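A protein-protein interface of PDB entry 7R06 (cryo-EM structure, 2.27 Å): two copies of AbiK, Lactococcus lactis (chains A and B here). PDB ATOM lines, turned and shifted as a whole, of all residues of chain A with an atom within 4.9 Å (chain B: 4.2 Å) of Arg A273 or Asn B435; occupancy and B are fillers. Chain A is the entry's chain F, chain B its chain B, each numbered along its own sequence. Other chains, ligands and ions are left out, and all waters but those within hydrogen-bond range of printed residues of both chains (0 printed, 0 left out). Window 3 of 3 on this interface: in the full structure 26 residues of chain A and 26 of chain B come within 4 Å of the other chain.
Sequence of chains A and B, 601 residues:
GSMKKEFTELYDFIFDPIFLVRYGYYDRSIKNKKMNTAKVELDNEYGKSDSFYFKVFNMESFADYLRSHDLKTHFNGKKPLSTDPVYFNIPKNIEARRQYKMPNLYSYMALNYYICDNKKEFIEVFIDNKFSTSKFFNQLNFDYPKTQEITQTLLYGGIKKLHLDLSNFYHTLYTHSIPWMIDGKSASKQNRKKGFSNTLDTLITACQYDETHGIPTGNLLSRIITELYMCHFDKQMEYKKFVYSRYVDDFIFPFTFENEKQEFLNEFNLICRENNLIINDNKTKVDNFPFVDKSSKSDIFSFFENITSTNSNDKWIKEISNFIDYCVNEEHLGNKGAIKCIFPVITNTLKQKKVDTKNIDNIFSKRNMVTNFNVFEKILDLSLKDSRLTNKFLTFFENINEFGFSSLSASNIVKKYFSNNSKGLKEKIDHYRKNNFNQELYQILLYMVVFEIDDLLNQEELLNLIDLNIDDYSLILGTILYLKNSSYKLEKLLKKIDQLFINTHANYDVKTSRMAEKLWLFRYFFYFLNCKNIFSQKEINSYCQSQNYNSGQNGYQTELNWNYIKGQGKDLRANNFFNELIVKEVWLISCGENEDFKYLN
The side-chain amide nitrogen (ND2) of Asn A266 lies close to the side-chain amide nitrogen (ND2) of Asn B435 (3.4 Å). O of Asn B435 is in hydrogen-bond range of NH2 of Arg A273 (2.9 Å). The backbone carbonyl oxygen of Asn B436 is in hydrogen-bond range of the guanidinium group of Arg A273.
The side-chain amide oxygen (OD1) of Asn B435 lies close to a ring nitrogen (NE2) of His B431 (3.3 Å).
Among the printed residues, pairs that only touch across the chains: Asn A266 with His B431, Leu A270 with Lys B434, Leu A270 with Asn B435, Leu A270 with Asn B436 and Arg A273 with Asn B89.
Printed residues of chain B within 4 Å of Asn A266: His B431 (3.8 Å) and Asn B435 (3.4 Å). Of the printed residues of chain A, Lys B434 touches Leu A270 (3.8 Å). Of chain A, only Asn A266, Leu A270 and Arg A273 come within 4 Å of Asn B435. Printed residues of chain A within 4 Å of Asn B436: Leu A270 (3.2 Å) and Arg A273 (3.2 Å). The nearest printed residue of chain A that does not touch His B431 is Leu A270 (7.9 Å).
Hydrophobic or aromatic side chains of chain A within 4 Å of the printed part of chain B: Leu A270. Of the 8 printed residues of chain B, 5 touch a printed residue of chain A. Along chain B the printed residues that touch a printed residue of chain A span positions 89 to 436. Among the printed residues, 8 pairs touch across the chains.
No position is printed for both chains.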
ATOM      1  N   LYS A 185       0.030  39.047  -0.266  1.00  0.00           N
ATOM      2  CA  LYS A 185       0.373  38.417   1.005  1.00  0.00           C
ATOM      3  C   LYS A 185       1.869  38.477   1.281  1.00  0.00           C
ATOM      4  O   LYS A 185       2.280  38.661   2.432  1.00  0.00           O
ATOM      5  CB  LYS A 185      -0.115  36.970   1.026  1.00  0.00           C
ATOM      6  CG  LYS A 185       0.126  36.253   2.343  1.00  0.00           C
ATOM      7  CD  LYS A 185      -0.301  34.802   2.256  1.00  0.00           C
ATOM      8  CE  LYS A 185      -0.546  34.215   3.630  1.00  0.00           C
ATOM      9  NZ  LYS A 185      -1.200  32.884   3.546  1.00  0.00           N
ATOM     10  N   ASN A 266     -10.348  25.567  -9.405  1.00  0.00           N
ATOM     11  CA  ASN A 266      -8.963  25.527  -8.941  1.00  0.00           C
ATOM     12  C   ASN A 266      -8.454  26.919  -8.580  1.00  0.00           C
ATOM     13  O   ASN A 266      -7.856  27.109  -7.515  1.00  0.00           O
ATOM     14  CB  ASN A 266      -8.046  24.870  -9.979  1.00  0.00           C
ATOM     15  CG  ASN A 266      -8.285  23.377 -10.116  1.00  0.00           C
ATOM     16  OD1 ASN A 266      -8.827  22.904 -11.106  1.00  0.00           O
ATOM     17  ND2 ASN A 266      -7.894  22.630  -9.097  1.00  0.00           N
ATOM     18  N   ASN A 269     -10.292  28.155  -5.355  1.00  0.00           N
ATOM     19  CA  ASN A 269      -9.738  27.431  -4.218  1.00  0.00           C
ATOM     20  C   ASN A 269      -8.365  27.967  -3.846  1.00  0.00           C
ATOM     21  O   ASN A 269      -8.041  28.100  -2.663  1.00  0.00           O
ATOM     22  CB  ASN A 269      -9.636  25.942  -4.550  1.00  0.00           C
ATOM     23  CG  ASN A 269     -10.972  25.243  -4.529  1.00  0.00           C
ATOM     24  OD1 ASN A 269     -11.854  25.589  -3.757  1.00  0.00           O
ATOM     25  ND2 ASN A 269     -11.132  24.254  -5.395  1.00  0.00           N
ATOM     26  N   LEU A 270      -7.540  28.270  -4.848  1.00  0.00           N
ATOM     27  CA  LEU A 270      -6.189  28.745  -4.582  1.00  0.00           C
ATOM     28  C   LEU A 270      -6.206  30.083  -3.851  1.00  0.00           C
ATOM     29  O   LEU A 270      -5.496  30.271  -2.857  1.00  0.00           O
ATOM     30  CB  LEU A 270      -5.424  28.855  -5.896  1.00  0.00           C
ATOM     31  CG  LEU A 270      -3.928  28.600  -5.821  1.00  0.00           C
ATOM     32  CD1 LEU A 270      -3.701  27.279  -5.123  1.00  0.00           C
ATOM     33  CD2 LEU A 270      -3.343  28.581  -7.213  1.00  0.00           C
ATOM     34  N   ILE A 271      -7.021  31.026  -4.327  1.00  0.00           N
ATOM     35  CA  ILE A 271      -7.082  32.330  -3.666  1.00  0.00           C
ATOM     36  C   ILE A 271      -7.696  32.210  -2.274  1.00  0.00           C
ATOM     37  O   ILE A 271      -7.237  32.857  -1.319  1.00  0.00           O
ATOM     38  CB  ILE A 271      -7.828  33.351  -4.543  1.00  0.00           C
ATOM     39  CG1 ILE A 271      -7.154  33.456  -5.907  1.00  0.00           C
ATOM     40  CG2 ILE A 271      -7.899  34.706  -3.873  1.00  0.00           C
ATOM     41  CD1 ILE A 271      -7.898  34.312  -6.871  1.00  0.00           C
ATOM     42  N   CYS A 272      -8.720  31.368  -2.125  1.00  0.00           N
ATOM     43  CA  CYS A 272      -9.316  31.168  -0.809  1.00  0.00           C
ATOM     44  C   CYS A 272      -8.308  30.579   0.173  1.00  0.00           C
ATOM     45  O   CYS A 272      -8.262  30.982   1.339  1.00  0.00           O
ATOM     46  CB  CYS A 272     -10.546  30.272  -0.923  1.00  0.00           C
ATOM     47  SG  CYS A 272     -12.011  31.121  -1.515  1.00  0.00           S
ATOM     48  N   ARG A 273      -7.492  29.627  -0.283  1.00  0.00           N
ATOM     49  CA  ARG A 273      -6.468  29.050   0.582  1.00  0.00           C
ATOM     50  C   ARG A 273      -5.398  30.076   0.923  1.00  0.00           C
ATOM     51  O   ARG A 273      -4.880  30.090   2.044  1.00  0.00           O
ATOM     52  CB  ARG A 273      -5.845  27.822  -0.080  1.00  0.00           C
ATOM     53  CG  ARG A 273      -6.607  26.543   0.184  1.00  0.00           C
ATOM     54  CD  ARG A 273      -5.940  25.321  -0.437  1.00  0.00           C
ATOM     55  NE  ARG A 273      -4.520  25.235  -0.116  1.00  0.00           N
ATOM     56  CZ  ARG A 273      -3.594  24.746  -0.935  1.00  0.00           C
ATOM     57  NH1 ARG A 273      -2.327  24.708  -0.551  1.00  0.00           N
ATOM     58  NH2 ARG A 273      -3.935  24.277  -2.126  1.00  0.00           N
ATOM     59  N   GLU A 274      -5.049  30.941  -0.031  1.00  0.00           N
ATOM     60  CA  GLU A 274      -4.056  31.969   0.258  1.00  0.00           C
ATOM     61  C   GLU A 274      -4.546  32.953   1.313  1.00  0.00           C
ATOM     62  O   GLU A 274      -3.742  33.462   2.098  1.00  0.00           O
ATOM     63  CB  GLU A 274      -3.677  32.719  -1.016  1.00  0.00           C
ATOM     64  CG  GLU A 274      -2.573  33.734  -0.802  1.00  0.00           C
ATOM     65  CD  GLU A 274      -2.272  34.560  -2.035  1.00  0.00           C
ATOM     66  OE1 GLU A 274      -2.909  34.331  -3.086  1.00  0.00           O
ATOM     67  OE2 GLU A 274      -1.396  35.446  -1.949  1.00  0.00           O
ATOM     68  N   ASN A 275      -5.847  33.234   1.357  1.00  0.00           N
ATOM     69  CA  ASN A 275      -6.353  34.276   2.241  1.00  0.00           C
ATOM     70  C   ASN A 275      -7.160  33.731   3.420  1.00  0.00           C
ATOM     71  O   ASN A 275      -7.900  34.486   4.053  1.00  0.00           O
ATOM     72  CB  ASN A 275      -7.174  35.280   1.435  1.00  0.00           C
ATOM     73  CG  ASN A 275      -6.305  36.160   0.562  1.00  0.00           C
ATOM     74  OD1 ASN A 275      -6.048  35.845  -0.595  1.00  0.00           O
ATOM     75  ND2 ASN A 275      -5.824  37.259   1.124  1.00  0.00           N
ATOM     76  N   ASN A 276      -7.013  32.444   3.739  1.00  0.00           N
ATOM     77  CA  ASN A 276      -7.742  31.803   4.841  1.00  0.00           C
ATOM     78  C   ASN A 276      -9.250  31.987   4.706  1.00  0.00           C
ATOM     79  O   ASN A 276      -9.951  32.264   5.679  1.00  0.00           O
ATOM     80  CB  ASN A 276      -7.264  32.300   6.207  1.00  0.00           C
ATOM     81  CG  ASN A 276      -5.802  32.007   6.458  1.00  0.00           C
ATOM     82  OD1 ASN A 276      -5.389  30.851   6.499  1.00  0.00           O
ATOM     83  ND2 ASN A 276      -5.015  33.052   6.655  1.00  0.00           N
ATOM     84  N   LEU A 277      -9.754  31.834   3.490  1.00  0.00           N
ATOM     85  CA  LEU A 277     -11.181  31.863   3.223  1.00  0.00           C
ATOM     86  C   LEU A 277     -11.665  30.435   3.014  1.00  0.00           C
ATOM     87  O   LEU A 277     -10.957  29.609   2.433  1.00  0.00           O
ATOM     88  CB  LEU A 277     -11.484  32.722   1.995  1.00  0.00           C
ATOM     89  CG  LEU A 277     -11.068  34.191   2.097  1.00  0.00           C
ATOM     90  CD1 LEU A 277     -11.300  34.914   0.781  1.00  0.00           C
ATOM     91  CD2 LEU A 277     -11.801  34.888   3.230  1.00  0.00           C
ATOM     92  N   ASN B  89       0.351  21.140   2.825  1.00  0.00           N
ATOM     93  CA  ASN B  89      -1.071  20.891   2.638  1.00  0.00           C
ATOM     94  C   ASN B  89      -1.294  19.431   2.262  1.00  0.00           C
ATOM     95  O   ASN B  89      -0.598  18.894   1.399  1.00  0.00           O
ATOM     96  CB  ASN B  89      -1.623  21.824   1.558  1.00  0.00           C
ATOM     97  CG  ASN B  89      -3.125  21.757   1.439  1.00  0.00           C
ATOM     98  OD1 ASN B  89      -3.664  20.934   0.704  1.00  0.00           O
ATOM     99  ND2 ASN B  89      -3.813  22.627   2.167  1.00  0.00           N
ATOM    100  N   HIS B 431      -0.180  19.047 -11.875  1.00  0.00           N
ATOM    101  CA  HIS B 431      -1.368  19.457 -11.134  1.00  0.00           C
ATOM    102  C   HIS B 431      -1.013  19.877  -9.715  1.00  0.00           C
ATOM    103  O   HIS B 431      -1.377  20.971  -9.270  1.00  0.00           O
ATOM    104  CB  HIS B 431      -2.381  18.320 -11.059  1.00  0.00           C
ATOM    105  CG  HIS B 431      -3.701  18.737 -10.492  1.00  0.00           C
ATOM    106  ND1 HIS B 431      -4.614  17.835  -9.997  1.00  0.00           N
ATOM    107  CD2 HIS B 431      -4.324  19.936 -10.483  1.00  0.00           C
ATOM    108  CE1 HIS B 431      -5.699  18.478  -9.605  1.00  0.00           C
ATOM    109  NE2 HIS B 431      -5.554  19.753  -9.901  1.00  0.00           N
ATOM    110  N   TYR B 432      -0.299  19.016  -8.984  1.00  0.00           N
ATOM    111  CA  TYR B 432       0.008  19.365  -7.602  1.00  0.00           C
ATOM    112  C   TYR B 432       0.993  20.513  -7.496  1.00  0.00           C
ATOM    113  O   TYR B 432       0.994  21.209  -6.478  1.00  0.00           O
ATOM    114  CB  TYR B 432       0.533  18.184  -6.777  1.00  0.00           C
ATOM    115  CG  TYR B 432      -0.057  16.828  -7.061  1.00  0.00           C
ATOM    116  CD1 TYR B 432      -1.424  16.620  -6.962  1.00  0.00           C
ATOM    117  CD2 TYR B 432       0.740  15.765  -7.450  1.00  0.00           C
ATOM    118  CE1 TYR B 432      -1.976  15.394  -7.217  1.00  0.00           C
ATOM    119  CE2 TYR B 432       0.195  14.527  -7.698  1.00  0.00           C
ATOM    120  CZ  TYR B 432      -1.168  14.350  -7.584  1.00  0.00           C
ATOM    121  OH  TYR B 432      -1.734  13.126  -7.834  1.00  0.00           O
ATOM    122  N   ARG B 433       1.814  20.739  -8.515  1.00  0.00           N
ATOM    123  CA  ARG B 433       2.706  21.888  -8.477  1.00  0.00           C
ATOM    124  C   ARG B 433       1.938  23.192  -8.662  1.00  0.00           C
ATOM    125  O   ARG B 433       2.175  24.160  -7.935  1.00  0.00           O
ATOM    126  CB  ARG B 433       3.802  21.720  -9.526  1.00  0.00           C
ATOM    127  CG  ARG B 433       5.170  21.988  -8.972  1.00  0.00           C
ATOM    128  CD  ARG B 433       6.275  21.310  -9.764  1.00  0.00           C
ATOM    129  NE  ARG B 433       6.109  21.348 -11.213  1.00  0.00           N
ATOM    130  CZ  ARG B 433       6.452  22.381 -11.972  1.00  0.00           C
ATOM    131  NH1 ARG B 433       6.285  22.327 -13.284  1.00  0.00           N
ATOM    132  NH2 ARG B 433       6.978  23.464 -11.418  1.00  0.00           N
ATOM    133  N   LYS B 434       1.001  23.235  -9.611  1.00  0.00           N
ATOM    134  CA  LYS B 434       0.197  24.445  -9.785  1.00  0.00           C
ATOM    135  C   LYS B 434      -0.725  24.705  -8.600  1.00  0.00           C
ATOM    136  O   LYS B 434      -0.939  25.861  -8.219  1.00  0.00           O
ATOM    137  CB  LYS B 434      -0.616  24.408 -11.086  1.00  0.00           C
ATOM    138  CG  LYS B 434       0.061  23.960 -12.391  1.00  0.00           C
ATOM    139  CD  LYS B 434       1.584  24.104 -12.400  1.00  0.00           C
ATOM    140  CE  LYS B 434       2.233  23.138 -13.359  1.00  0.00           C
ATOM    141  NZ  LYS B 434       3.701  23.269 -13.340  1.00  0.00           N
ATOM    142  N   ASN B 435      -1.291  23.660  -8.008  1.00  0.00           N
ATOM    143  CA  ASN B 435      -2.347  23.839  -7.024  1.00  0.00           C
ATOM    144  C   ASN B 435      -1.878  23.657  -5.586  1.00  0.00           C
ATOM    145  O   ASN B 435      -2.713  23.601  -4.681  1.00  0.00           O
ATOM    146  CB  ASN B 435      -3.494  22.891  -7.345  1.00  0.00           C
ATOM    147  CG  ASN B 435      -4.283  23.337  -8.550  1.00  0.00           C
ATOM    148  OD1 ASN B 435      -4.225  22.717  -9.607  1.00  0.00           O
ATOM    149  ND2 ASN B 435      -5.038  24.412  -8.394  1.00  0.00           N
ATOM    150  N   ASN B 436      -0.567  23.593  -5.355  1.00  0.00           N
ATOM    151  CA  ASN B 436       0.002  23.450  -4.012  1.00  0.00           C
ATOM    152  C   ASN B 436      -0.566  22.244  -3.266  1.00  0.00           C
ATOM    153  O   ASN B 436      -0.917  22.331  -2.090  1.00  0.00           O
ATOM    154  CB  ASN B 436      -0.184  24.728  -3.186  1.00  0.00           C
ATOM    155  CG  ASN B 436       0.310  25.960  -3.899  1.00  0.00           C
ATOM    156  OD1 ASN B 436       1.508  26.168  -4.027  1.00  0.00           O
ATOM    157  ND2 ASN B 436      -0.608  26.803  -4.339  1.00  0.00           N
ATOM    158  N   PHE B 437      -0.664  21.104  -3.951  1.00  0.00           N
ATOM    159  CA  PHE B 437      -1.021  19.849  -3.285  1.00  0.00           C
ATOM    160  C   PHE B 437       0.290  19.262  -2.778  1.00  0.00           C
ATOM    161  O   PHE B 437       0.954  18.501  -3.479  1.00  0.00           O
ATOM    162  CB  PHE B 437      -1.696  18.859  -4.224  1.00  0.00           C
ATOM    163  CG  PHE B 437      -3.098  19.211  -4.623  1.00  0.00           C
ATOM    164  CD1 PHE B 437      -4.150  19.061  -3.761  1.00  0.00           C
ATOM    165  CD2 PHE B 437      -3.354  19.725  -5.869  1.00  0.00           C
ATOM    166  CE1 PHE B 437      -5.444  19.385  -4.148  1.00  0.00           C
ATOM    167  CE2 PHE B 437      -4.636  20.031  -6.254  1.00  0.00           C
ATOM    168  CZ  PHE B 437      -5.678  19.879  -5.389  1.00  0.00           C
